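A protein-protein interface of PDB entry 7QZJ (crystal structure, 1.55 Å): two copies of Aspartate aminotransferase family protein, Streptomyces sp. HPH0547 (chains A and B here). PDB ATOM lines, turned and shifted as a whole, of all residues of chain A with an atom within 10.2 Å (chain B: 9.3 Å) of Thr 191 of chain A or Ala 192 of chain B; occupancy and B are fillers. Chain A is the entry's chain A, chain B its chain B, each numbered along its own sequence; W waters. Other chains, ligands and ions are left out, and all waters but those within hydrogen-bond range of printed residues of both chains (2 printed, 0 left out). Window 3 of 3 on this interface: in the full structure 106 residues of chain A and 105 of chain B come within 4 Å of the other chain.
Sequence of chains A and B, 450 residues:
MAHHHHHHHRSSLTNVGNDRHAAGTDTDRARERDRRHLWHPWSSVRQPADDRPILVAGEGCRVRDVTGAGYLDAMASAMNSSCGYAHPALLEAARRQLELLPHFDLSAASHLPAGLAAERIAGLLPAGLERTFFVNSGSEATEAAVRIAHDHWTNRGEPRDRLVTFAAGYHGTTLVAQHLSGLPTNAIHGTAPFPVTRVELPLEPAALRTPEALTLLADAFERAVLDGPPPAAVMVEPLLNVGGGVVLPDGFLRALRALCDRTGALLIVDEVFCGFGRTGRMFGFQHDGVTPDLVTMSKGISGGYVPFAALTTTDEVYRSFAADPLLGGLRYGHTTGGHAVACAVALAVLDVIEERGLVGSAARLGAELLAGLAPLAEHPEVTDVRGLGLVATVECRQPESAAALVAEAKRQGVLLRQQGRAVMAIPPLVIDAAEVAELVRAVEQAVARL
A ring nitrogen (ND1) of His 189 of chain A lies within hydrogen-bond range of a ring nitrogen (ND1) of His 150 of chain B. The backbone carbonyl oxygen of Pro 193 of chain A lies within hydrogen-bond range of the backbone NH of Thr 191 of chain B (2.8 Å). The backbone carbonyl oxygen (O) of Pro 193 of chain B sits at hydrogen-bond distance from the backbone NH (N) of Thr 191 of chain A (2.8 Å).
NE2 of His 150 of chain B lies within hydrogen-bond range of O of Asp 161 of chain B (2.8 Å).
Hydrophobic or aromatic side chains of chain A that line the printed part of chain B: Leu 175, Val 176, His 189 and Pro 193. Printed residues of chain B that touch a printed residue of chain A: His 150, Leu 175, Val 176, Gly 190, Thr 191, Ala 192 and Pro 193. Hydrophobic or aromatic side chains of chain B within 4 Å of the printed part of chain A: His 150, Leu 175, Val 176 and Pro 193. Among the printed residues, 9 pairs touch across the chains. Among the printed residues, no Asp or Glu carboxylate lies within 4 Å of a Lys or Arg side-chain nitrogen of the other chain.
Water W1 bridges O of His 189 of chain A (2.8 Å) and NE2 of His 150 of chain B (3.3 Å). Water W2 bridges N of Val 176 of chain A (3.2 Å) and N of Val 176 of chain B (3.4 Å).
Among the printed residues, pairs that only touch across the chains: Leu 175 of chain A with Val 176 of chain B, Val 176 of chain A with Leu 175 of chain B, Gly 190 of chain A with Pro 193 of chain B, Thr 191 of chain A with Ala 192 of chain B, Ala 192 of chain A with Thr 191 of chain B and Pro 193 of chain A with Gly 190 of chain B.
Leu 175 of chain A touches Val 176 of chain B, and with the chains exchanged Val 176 of chain A touches Leu 175 of chain B. Gly 190 of chain A touches Pro 193 of chain B, and with the chains exchanged Pro 193 of chain A touches Gly 190 of chain B. Thr 191 of chain A touches Ala 192 of chain B, and with the chains exchanged Ala 192 of chain A touches Thr 191 of chain B. Thr 191 of chain A touches Pro 193 of chain B, and with the chains exchanged Pro 193 of chain A touches Thr 191 of chain B. Of the 9 pairs that touch across the chains among the printed residues, 8 have their exchanged pair printed and touching as well.
Of chain B, only Ala 192 and Pro 193 come within 4 Å of Thr 191 of chain A. Of chain A, only Thr 191 comes within 4 Å of Ala 192 of chain B. Of chain B, only Pro 193 comes within 4 Å of Gly 190 of chain A. Of chain B, only Thr 191 (3.7 Å) comes within 4 Å of Ala 192 of chain A. Of chain A, only Ala 192 and Pro 193 come within 4 Å of Thr 191 of chain B. Of the printed residues of chain A, Val 176 of chain B touches Leu 175 (3.5 Å). Printed residues of chain B within 4 Å of Leu 175 of chain A: Val 176 (3.5 Å). Printed residues of chain B within 4 Å of Val 176 of chain A: Leu 175 (3.6 Å). Printed residues of chain B within 4 Å of Pro 193 of chain A: Gly 190 (3.3 Å) and Thr 191 (2.8 Å). Printed residues of chain A within 4 Å of Leu 175 of chain B: Val 176. The nearest residue of chain B that does not touch Thr 191 of chain A is Phe 194 of chain B (4.6 Å). The nearest residue of chain A that does not touch Ala 192 of chain B is Ala 192 of chain A (4.8 Å).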
ATOM      1  N   LEU A 175      15.844   2.249  17.665  1.00  0.00           N
ATOM      2  CA  LEU A 175      15.728   3.712  17.835  1.00  0.00           C
ATOM      3  C   LEU A 175      15.938   4.101  19.293  1.00  0.00           C
ATOM      4  O   LEU A 175      16.691   5.041  19.579  1.00  0.00           O
ATOM      5  CB  LEU A 175      14.396   4.260  17.308  1.00  0.00           C
ATOM      6  CG  LEU A 175      14.258   5.800  17.378  1.00  0.00           C
ATOM      7  CD1 LEU A 175      13.504   6.378  16.191  1.00  0.00           C
ATOM      8  CD2 LEU A 175      13.571   6.246  18.654  1.00  0.00           C
ATOM      9  N   VAL A 176      15.294   3.404  20.210  1.00  0.00           N
ATOM     10  CA  VAL A 176      15.448   3.731  21.637  1.00  0.00           C
ATOM     11  C   VAL A 176      16.882   3.501  22.087  1.00  0.00           C
ATOM     12  O   VAL A 176      17.462   4.339  22.796  1.00  0.00           O
ATOM     13  CB  VAL A 176      14.441   2.970  22.504  1.00  0.00           C
ATOM     14  CG1 VAL A 176      14.826   2.996  23.973  1.00  0.00           C
ATOM     15  CG2 VAL A 176      13.064   3.592  22.318  1.00  0.00           C
ATOM     16  N   GLN A 178      19.686   3.531  20.300  1.00  0.00           N
ATOM     17  CA  GLN A 178      20.539   4.534  19.673  1.00  0.00           C
ATOM     18  C   GLN A 178      20.317   5.910  20.313  1.00  0.00           C
ATOM     19  O   GLN A 178      21.263   6.676  20.441  1.00  0.00           O
ATOM     20  CB  GLN A 178      20.316   4.612  18.162  1.00  0.00           C
ATOM     21  CG  GLN A 178      20.866   3.397  17.445  1.00  0.00           C
ATOM     22  CD  GLN A 178      20.621   3.458  15.947  1.00  0.00           C
ATOM     23  OE1 GLN A 178      19.521   3.795  15.505  1.00  0.00           O
ATOM     24  NE2 GLN A 178      21.610   3.093  15.169  1.00  0.00           N
ATOM     25  N   HIS A 179      19.075   6.218  20.697  1.00  0.00           N
ATOM     26  CA  HIS A 179      18.760   7.506  21.342  1.00  0.00           C
ATOM     27  C   HIS A 179      19.525   7.706  22.667  1.00  0.00           C
ATOM     28  O   HIS A 179      19.883   8.835  23.026  1.00  0.00           O
ATOM     29  CB  HIS A 179      17.263   7.581  21.577  1.00  0.00           C
ATOM     30  CG  HIS A 179      16.809   8.865  22.181  1.00  0.00           C
ATOM     31  ND1 HIS A 179      17.122  10.097  21.640  1.00  0.00           N
ATOM     32  CD2 HIS A 179      16.070   9.101  23.282  1.00  0.00           C
ATOM     33  CE1 HIS A 179      16.598  11.039  22.409  1.00  0.00           C
ATOM     34  NE2 HIS A 179      15.941  10.461  23.395  1.00  0.00           N
ATOM     35  N   LEU A 180      19.812   6.625  23.368  1.00  0.00           N
ATOM     36  CA  LEU A 180      20.589   6.703  24.616  1.00  0.00           C
ATOM     37  C   LEU A 180      22.032   7.118  24.373  1.00  0.00           C
ATOM     38  O   LEU A 180      22.670   7.678  25.266  1.00  0.00           O
ATOM     39  CB  LEU A 180      20.600   5.353  25.323  1.00  0.00           C
ATOM     40  CG  LEU A 180      19.258   4.807  25.760  1.00  0.00           C
ATOM     41  CD1 LEU A 180      19.440   3.492  26.501  1.00  0.00           C
ATOM     42  CD2 LEU A 180      18.525   5.792  26.630  1.00  0.00           C
ATOM     43  N   ALA A 187      22.988   8.640  15.391  1.00  0.00           N
ATOM     44  CA  ALA A 187      21.939   9.617  15.162  1.00  0.00           C
ATOM     45  C   ALA A 187      20.645   8.900  14.753  1.00  0.00           C
ATOM     46  O   ALA A 187      20.649   8.065  13.838  1.00  0.00           O
ATOM     47  CB  ALA A 187      22.357  10.600  14.085  1.00  0.00           C
ATOM     48  N   ILE A 188      19.564   9.204  15.451  1.00  0.00           N
ATOM     49  CA  ILE A 188      18.288   8.515  15.221  1.00  0.00           C
ATOM     50  C   ILE A 188      17.551   9.066  14.008  1.00  0.00           C
ATOM     51  O   ILE A 188      17.781  10.195  13.586  1.00  0.00           O
ATOM     52  CB  ILE A 188      17.371   8.519  16.461  1.00  0.00           C
ATOM     53  CG1 ILE A 188      16.952   9.939  16.876  1.00  0.00           C
ATOM     54  CG2 ILE A 188      18.053   7.814  17.624  1.00  0.00           C
ATOM     55  CD1 ILE A 188      15.786   9.941  17.818  1.00  0.00           C
ATOM     56  N   HIS A 189      16.656   8.241  13.464  1.00  0.00           N
ATOM     57  CA  HIS A 189      15.821   8.587  12.302  1.00  0.00           C
ATOM     58  C   HIS A 189      14.443   9.162  12.622  1.00  0.00           C
ATOM     59  O   HIS A 189      13.576   9.214  11.752  1.00  0.00           O
ATOM     60  CB  HIS A 189      15.633   7.359  11.397  1.00  0.00           C
ATOM     61  CG  HIS A 189      14.995   6.187  12.080  1.00  0.00           C
ATOM     62  ND1 HIS A 189      13.644   5.938  12.030  1.00  0.00           N
ATOM     63  CD2 HIS A 189      15.534   5.171  12.793  1.00  0.00           C
ATOM     64  CE1 HIS A 189      13.370   4.839  12.702  1.00  0.00           C
ATOM     65  NE2 HIS A 189      14.499   4.348  13.173  1.00  0.00           N
ATOM     66  N   GLY A 190      14.208   9.588  13.838  1.00  0.00           N
ATOM     67  CA  GLY A 190      12.987  10.358  14.117  1.00  0.00           C
ATOM     68  C   GLY A 190      13.373  11.444  15.073  1.00  0.00           C
ATOM     69  O   GLY A 190      14.528  11.874  15.074  1.00  0.00           O
ATOM     70  N   THR A 191      12.428  11.852  15.899  1.00  0.00           N
ATOM     71  CA  THR A 191      12.674  12.809  16.958  1.00  0.00           C
ATOM     72  C   THR A 191      12.649  12.096  18.300  1.00  0.00           C
ATOM     73  O   THR A 191      12.216  10.944  18.426  1.00  0.00           O
ATOM     74  CB  THR A 191      11.647  13.946  16.958  1.00  0.00           C
ATOM     75  OG1 THR A 191      10.337  13.399  17.100  1.00  0.00           O
ATOM     76  CG2 THR A 191      11.726  14.762  15.660  1.00  0.00           C
ATOM     77  N   ALA A 192      13.129  12.788  19.330  1.00  0.00           N
ATOM     78  CA  ALA A 192      13.341  12.152  20.623  1.00  0.00           C
ATOM     79  C   ALA A 192      12.083  11.611  21.284  1.00  0.00           C
ATOM     80  O   ALA A 192      11.152  12.362  21.551  1.00  0.00           O
ATOM     81  CB  ALA A 192      14.028  13.141  21.569  1.00  0.00           C
ATOM     82  N   PRO A 193      12.038  10.306  21.586  1.00  0.00           N
ATOM     83  CA  PRO A 193      10.860   9.769  22.256  1.00  0.00           C
ATOM     84  C   PRO A 193      10.760  10.055  23.754  1.00  0.00           C
ATOM     85  O   PRO A 193       9.702   9.850  24.350  1.00  0.00           O
ATOM     86  CB  PRO A 193      10.975   8.255  21.988  1.00  0.00           C
ATOM     87  CG  PRO A 193      12.413   8.011  21.769  1.00  0.00           C
ATOM     88  CD  PRO A 193      12.964   9.242  21.141  1.00  0.00           C
ATOM     89  N   PHE A 194      11.871  10.496  24.343  1.00  0.00           N
ATOM     90  CA  PHE A 194      11.927  10.910  25.736  1.00  0.00           C
ATOM     91  C   PHE A 194      13.239  11.647  25.934  1.00  0.00           C
ATOM     92  O   PHE A 194      14.162  11.509  25.128  1.00  0.00           O
ATOM     93  CB  PHE A 194      11.849   9.703  26.678  1.00  0.00           C
ATOM     94  CG  PHE A 194      12.854   8.637  26.390  1.00  0.00           C
ATOM     95  CD1 PHE A 194      14.115   8.642  26.997  1.00  0.00           C
ATOM     96  CD2 PHE A 194      12.538   7.591  25.536  1.00  0.00           C
ATOM     97  CE1 PHE A 194      15.043   7.645  26.731  1.00  0.00           C
ATOM     98  CE2 PHE A 194      13.456   6.587  25.281  1.00  0.00           C
ATOM     99  CZ  PHE A 194      14.712   6.607  25.872  1.00  0.00           C
ATOM    100  N   PRO A 195      13.321  12.476  26.987  1.00  0.00           N
ATOM    101  CA  PRO A 195      14.564  13.215  27.168  1.00  0.00           C
ATOM    102  C   PRO A 195      15.702  12.329  27.689  1.00  0.00           C
ATOM    103  O   PRO A 195      15.450  11.467  28.544  1.00  0.00           O
ATOM    104  CB  PRO A 195      14.206  14.303  28.179  1.00  0.00           C
ATOM    105  CG  PRO A 195      12.788  14.103  28.543  1.00  0.00           C
ATOM    106  CD  PRO A 195      12.276  12.830  27.958  1.00  0.00           C
ATOM    107  N   VAL A 196      16.905  12.548  27.162  1.00  0.00           N
ATOM    108  CA  VAL A 196      18.114  11.892  27.682  1.00  0.00           C
ATOM    109  C   VAL A 196      19.171  12.958  27.946  1.00  0.00           C
ATOM    110  O   VAL A 196      19.351  13.859  27.148  1.00  0.00           O
ATOM    111  CB  VAL A 196      18.665  10.831  26.695  1.00  0.00           C
ATOM    112  CG1 VAL A 196      19.829  10.057  27.301  1.00  0.00           C
ATOM    113  CG2 VAL A 196      17.587   9.842  26.305  1.00  0.00           C
ATOM    114  N   ARG A 198      23.055  13.101  28.230  1.00  0.00           N
ATOM    115  CA  ARG A 198      24.197  12.257  27.889  1.00  0.00           C
ATOM    116  C   ARG A 198      25.460  12.945  28.377  1.00  0.00           C
ATOM    117  O   ARG A 198      25.818  14.022  27.866  1.00  0.00           O
ATOM    118  CB  ARG A 198      24.267  12.041  26.393  1.00  0.00           C
ATOM    119  CG  ARG A 198      22.978  11.502  25.806  1.00  0.00           C
ATOM    120  CD  ARG A 198      23.176  11.156  24.347  1.00  0.00           C
ATOM    121  NE  ARG A 198      21.910  10.926  23.657  1.00  0.00           N
ATOM    122  CZ  ARG A 198      21.021  11.857  23.321  1.00  0.00           C
ATOM    123  NH1 ARG A 198      21.205  13.148  23.611  1.00  0.00           N
ATOM    124  NH2 ARG A 198      19.901  11.501  22.695  1.00  0.00           N
ATOM    125  N   HIS B 150      12.726   5.869   6.452  1.00  0.00           N
ATOM    126  CA  HIS B 150      13.066   7.277   6.747  1.00  0.00           C
ATOM    127  C   HIS B 150      14.376   7.682   6.093  1.00  0.00           C
ATOM    128  O   HIS B 150      14.467   8.741   5.436  1.00  0.00           O
ATOM    129  CB  HIS B 150      13.172   7.509   8.260  1.00  0.00           C
ATOM    130  CG  HIS B 150      11.851   7.585   8.961  1.00  0.00           C
ATOM    131  ND1 HIS B 150      11.684   7.201  10.269  1.00  0.00           N
ATOM    132  CD2 HIS B 150      10.638   8.009   8.548  1.00  0.00           C
ATOM    133  CE1 HIS B 150      10.437   7.404  10.646  1.00  0.00           C
ATOM    134  NE2 HIS B 150       9.774   7.884   9.614  1.00  0.00           N
ATOM    135  N   ASP B 161       8.745  11.777   7.025  1.00  0.00           N
ATOM    136  CA  ASP B 161       8.694  11.184   8.351  1.00  0.00           C
ATOM    137  C   ASP B 161       7.484  10.293   8.645  1.00  0.00           C
ATOM    138  O   ASP B 161       7.520   9.492   9.583  1.00  0.00           O
ATOM    139  CB  ASP B 161       8.851  12.265   9.446  1.00  0.00           C
ATOM    140  CG  ASP B 161       7.772  13.315   9.438  1.00  0.00           C
ATOM    141  OD1 ASP B 161       6.965  13.399   8.502  1.00  0.00           O
ATOM    142  OD2 ASP B 161       7.757  14.124  10.399  1.00  0.00           O
ATOM    143  N   LEU B 175       9.744   0.034  20.914  1.00  0.00           N
ATOM    144  CA  LEU B 175       8.970   1.284  20.899  1.00  0.00           C
ATOM    145  C   LEU B 175       8.499   1.689  19.512  1.00  0.00           C
ATOM    146  O   LEU B 175       7.330   2.046  19.323  1.00  0.00           O
ATOM    147  CB  LEU B 175       9.766   2.412  21.583  1.00  0.00           C
ATOM    148  CG  LEU B 175       9.030   3.760  21.685  1.00  0.00           C
ATOM    149  CD1 LEU B 175       9.355   4.476  22.999  1.00  0.00           C
ATOM    150  CD2 LEU B 175       9.335   4.666  20.505  1.00  0.00           C
ATOM    151  N   VAL B 176       9.391   1.619  18.529  1.00  0.00           N
ATOM    152  CA  VAL B 176       9.013   1.962  17.166  1.00  0.00           C
ATOM    153  C   VAL B 176       7.928   1.006  16.638  1.00  0.00           C
ATOM    154  O   VAL B 176       6.941   1.451  16.065  1.00  0.00           O
ATOM    155  CB  VAL B 176      10.219   2.047  16.213  1.00  0.00           C
ATOM    156  CG1 VAL B 176       9.803   2.108  14.741  1.00  0.00           C
ATOM    157  CG2 VAL B 176      11.114   3.230  16.565  1.00  0.00           C
ATOM    158  N   HIS B 179       4.671   1.750  18.283  1.00  0.00           N
ATOM    159  CA  HIS B 179       4.136   3.041  17.834  1.00  0.00           C
ATOM    160  C   HIS B 179       3.335   2.920  16.530  1.00  0.00           C
ATOM    161  O   HIS B 179       2.361   3.656  16.320  1.00  0.00           O
ATOM    162  CB  HIS B 179       5.279   4.035  17.700  1.00  0.00           C
ATOM    163  CG  HIS B 179       4.862   5.399  17.265  1.00  0.00           C
ATOM    164  ND1 HIS B 179       3.917   6.146  17.934  1.00  0.00           N
ATOM    165  CD2 HIS B 179       5.271   6.154  16.221  1.00  0.00           C
ATOM    166  CE1 HIS B 179       3.759   7.303  17.317  1.00  0.00           C
ATOM    167  NE2 HIS B 179       4.571   7.335  16.279  1.00  0.00           N
ATOM    168  N   LEU B 180       3.720   1.975  15.674  1.00  0.00           N
ATOM    169  CA  LEU B 180       2.986   1.770  14.421  1.00  0.00           C
ATOM    170  C   LEU B 180       1.560   1.240  14.667  1.00  0.00           C
ATOM    171  O   LEU B 180       0.672   1.453  13.865  1.00  0.00           O
ATOM    172  CB  LEU B 180       3.758   0.784  13.528  1.00  0.00           C
ATOM    173  CG  LEU B 180       5.125   1.212  13.066  1.00  0.00           C
ATOM    174  CD1 LEU B 180       5.753   0.131  12.205  1.00  0.00           C
ATOM    175  CD2 LEU B 180       5.095   2.525  12.313  1.00  0.00           C
ATOM    176  N   ILE B 188       2.771   3.249  23.794  1.00  0.00           N
ATOM    177  CA  ILE B 188       4.214   3.408  23.983  1.00  0.00           C
ATOM    178  C   ILE B 188       4.528   4.124  25.295  1.00  0.00           C
ATOM    179  O   ILE B 188       3.677   4.833  25.832  1.00  0.00           O
ATOM    180  CB  ILE B 188       4.910   4.098  22.800  1.00  0.00           C
ATOM    181  CG1 ILE B 188       4.433   5.540  22.594  1.00  0.00           C
ATOM    182  CG2 ILE B 188       4.761   3.254  21.540  1.00  0.00           C
ATOM    183  CD1 ILE B 188       5.301   6.328  21.645  1.00  0.00           C
ATOM    184  N   HIS B 189       5.760   3.947  25.764  1.00  0.00           N
ATOM    185  CA  HIS B 189       6.272   4.546  26.997  1.00  0.00           C
ATOM    186  C   HIS B 189       7.056   5.847  26.790  1.00  0.00           C
ATOM    187  O   HIS B 189       7.918   6.199  27.589  1.00  0.00           O
ATOM    188  CB  HIS B 189       7.130   3.537  27.763  1.00  0.00           C
ATOM    189  CG  HIS B 189       8.296   3.008  26.983  1.00  0.00           C
ATOM    190  ND1 HIS B 189       9.541   3.589  27.010  1.00  0.00           N
ATOM    191  CD2 HIS B 189       8.401   1.946  26.148  1.00  0.00           C
ATOM    192  CE1 HIS B 189      10.368   2.904  26.235  1.00  0.00           C
ATOM    193  NE2 HIS B 189       9.695   1.902  25.702  1.00  0.00           N
ATOM    194  N   GLY B 190       6.777   6.567  25.723  1.00  0.00           N
ATOM    195  CA  GLY B 190       7.346   7.891  25.550  1.00  0.00           C
ATOM    196  C   GLY B 190       6.403   8.643  24.663  1.00  0.00           C
ATOM    197  O   GLY B 190       5.211   8.331  24.616  1.00  0.00           O
ATOM    198  N   THR B 191       6.932   9.619  23.946  1.00  0.00           N
ATOM    199  CA  THR B 191       6.156  10.365  22.982  1.00  0.00           C
ATOM    200  C   THR B 191       6.527   9.940  21.558  1.00  0.00           C
ATOM    201  O   THR B 191       7.560   9.290  21.335  1.00  0.00           O
ATOM    202  CB  THR B 191       6.352  11.869  23.153  1.00  0.00           C
ATOM    203  OG1 THR B 191       7.723  12.192  22.951  1.00  0.00           O
ATOM    204  CG2 THR B 191       5.911  12.291  24.543  1.00  0.00           C
ATOM    205  N   ALA B 192       5.682  10.333  20.613  1.00  0.00           N
ATOM    206  CA  ALA B 192       5.803   9.880  19.234  1.00  0.00           C
ATOM    207  C   ALA B 192       7.141  10.273  18.611  1.00  0.00           C
ATOM    208  O   ALA B 192       7.464  11.450  18.547  1.00  0.00           O
ATOM    209  CB  ALA B 192       4.654  10.440  18.405  1.00  0.00           C
ATOM    210  N   PRO B 193       7.945   9.295  18.133  1.00  0.00           N
ATOM    211  CA  PRO B 193       9.210   9.642  17.452  1.00  0.00           C
ATOM    212  C   PRO B 193       9.073  10.071  15.994  1.00  0.00           C
ATOM    213  O   PRO B 193      10.039  10.538  15.368  1.00  0.00           O
ATOM    214  CB  PRO B 193      10.039   8.345  17.570  1.00  0.00           C
ATOM    215  CG  PRO B 193       9.041   7.289  17.683  1.00  0.00           C
ATOM    216  CD  PRO B 193       7.849   7.849  18.402  1.00  0.00           C
ATOM    217  N   PHE B 194       7.882   9.862  15.440  1.00  0.00           N
ATOM    218  CA  PHE B 194       7.529  10.294  14.098  1.00  0.00           C
ATOM    219  C   PHE B 194       6.021  10.160  13.956  1.00  0.00           C
ATOM    220  O   PHE B 194       5.384   9.424  14.716  1.00  0.00           O
ATOM    221  CB  PHE B 194       8.246   9.496  13.005  1.00  0.00           C
ATOM    222  CG  PHE B 194       8.090   8.011  13.130  1.00  0.00           C
ATOM    223  CD1 PHE B 194       8.971   7.280  13.914  1.00  0.00           C
ATOM    224  CD2 PHE B 194       7.080   7.347  12.476  1.00  0.00           C
ATOM    225  CE1 PHE B 194       8.835   5.902  14.022  1.00  0.00           C
ATOM    226  CE2 PHE B 194       6.923   5.978  12.608  1.00  0.00           C
ATOM    227  CZ  PHE B 194       7.804   5.252  13.375  1.00  0.00           C
ATOM    228  N   PRO B 195       5.426  10.881  13.000  1.00  0.00           N
ATOM    229  CA  PRO B 195       3.982  10.802  12.854  1.00  0.00           C
ATOM    230  C   PRO B 195       3.544   9.480  12.216  1.00  0.00           C
ATOM    231  O   PRO B 195       4.202   9.007  11.281  1.00  0.00           O
ATOM    232  CB  PRO B 195       3.640  11.962  11.901  1.00  0.00           C
ATOM    233  CG  PRO B 195       4.881  12.648  11.609  1.00  0.00           C
ATOM    234  CD  PRO B 195       6.039  11.862  12.092  1.00  0.00           C
ATOM    235  N   VAL B 196       2.467   8.903  12.727  1.00  0.00           N
ATOM    236  CA  VAL B 196       1.833   7.731  12.121  1.00  0.00           C
ATOM    237  C   VAL B 196       0.340   8.004  11.967  1.00  0.00           C
ATOM    238  O   VAL B 196      -0.279   8.559  12.875  1.00  0.00           O
ATOM    239  CB  VAL B 196       2.063   6.467  12.963  1.00  0.00           C
ATOM    240  CG1 VAL B 196       1.486   5.217  12.296  1.00  0.00           C
ATOM    241  CG2 VAL B 196       3.546   6.253  13.194  1.00  0.00           C
ATOM    242  N   ARG B 198      -2.942   5.940  11.515  1.00  0.00           N
ATOM    243  CA  ARG B 198      -3.376   4.550  11.712  1.00  0.00           C
ATOM    244  C   ARG B 198      -4.834   4.430  11.271  1.00  0.00           C
ATOM    245  O   ARG B 198      -5.712   5.131  11.785  1.00  0.00           O
ATOM    246  CB  ARG B 198      -3.207   4.146  13.164  1.00  0.00           C
ATOM    247  CG  ARG B 198      -1.829   4.400  13.764  1.00  0.00           C
ATOM    248  CD  ARG B 198      -1.757   3.861  15.188  1.00  0.00           C
ATOM    249  NE  ARG B 198      -0.558   4.314  15.886  1.00  0.00           N
ATOM    250  CZ  ARG B 198      -0.383   5.523  16.406  1.00  0.00           C
ATOM    251  NH1 ARG B 198      -1.352   6.463  16.329  1.00  0.00           N
ATOM    252  NH2 ARG B 198       0.782   5.819  16.997  1.00  0.00           N
HETATM  253  O   HOH W   1      11.439  10.591  10.663  1.00  0.00           O
HETATM  254  O   HOH W   2      12.702   1.756  19.340  1.00  0.00           O
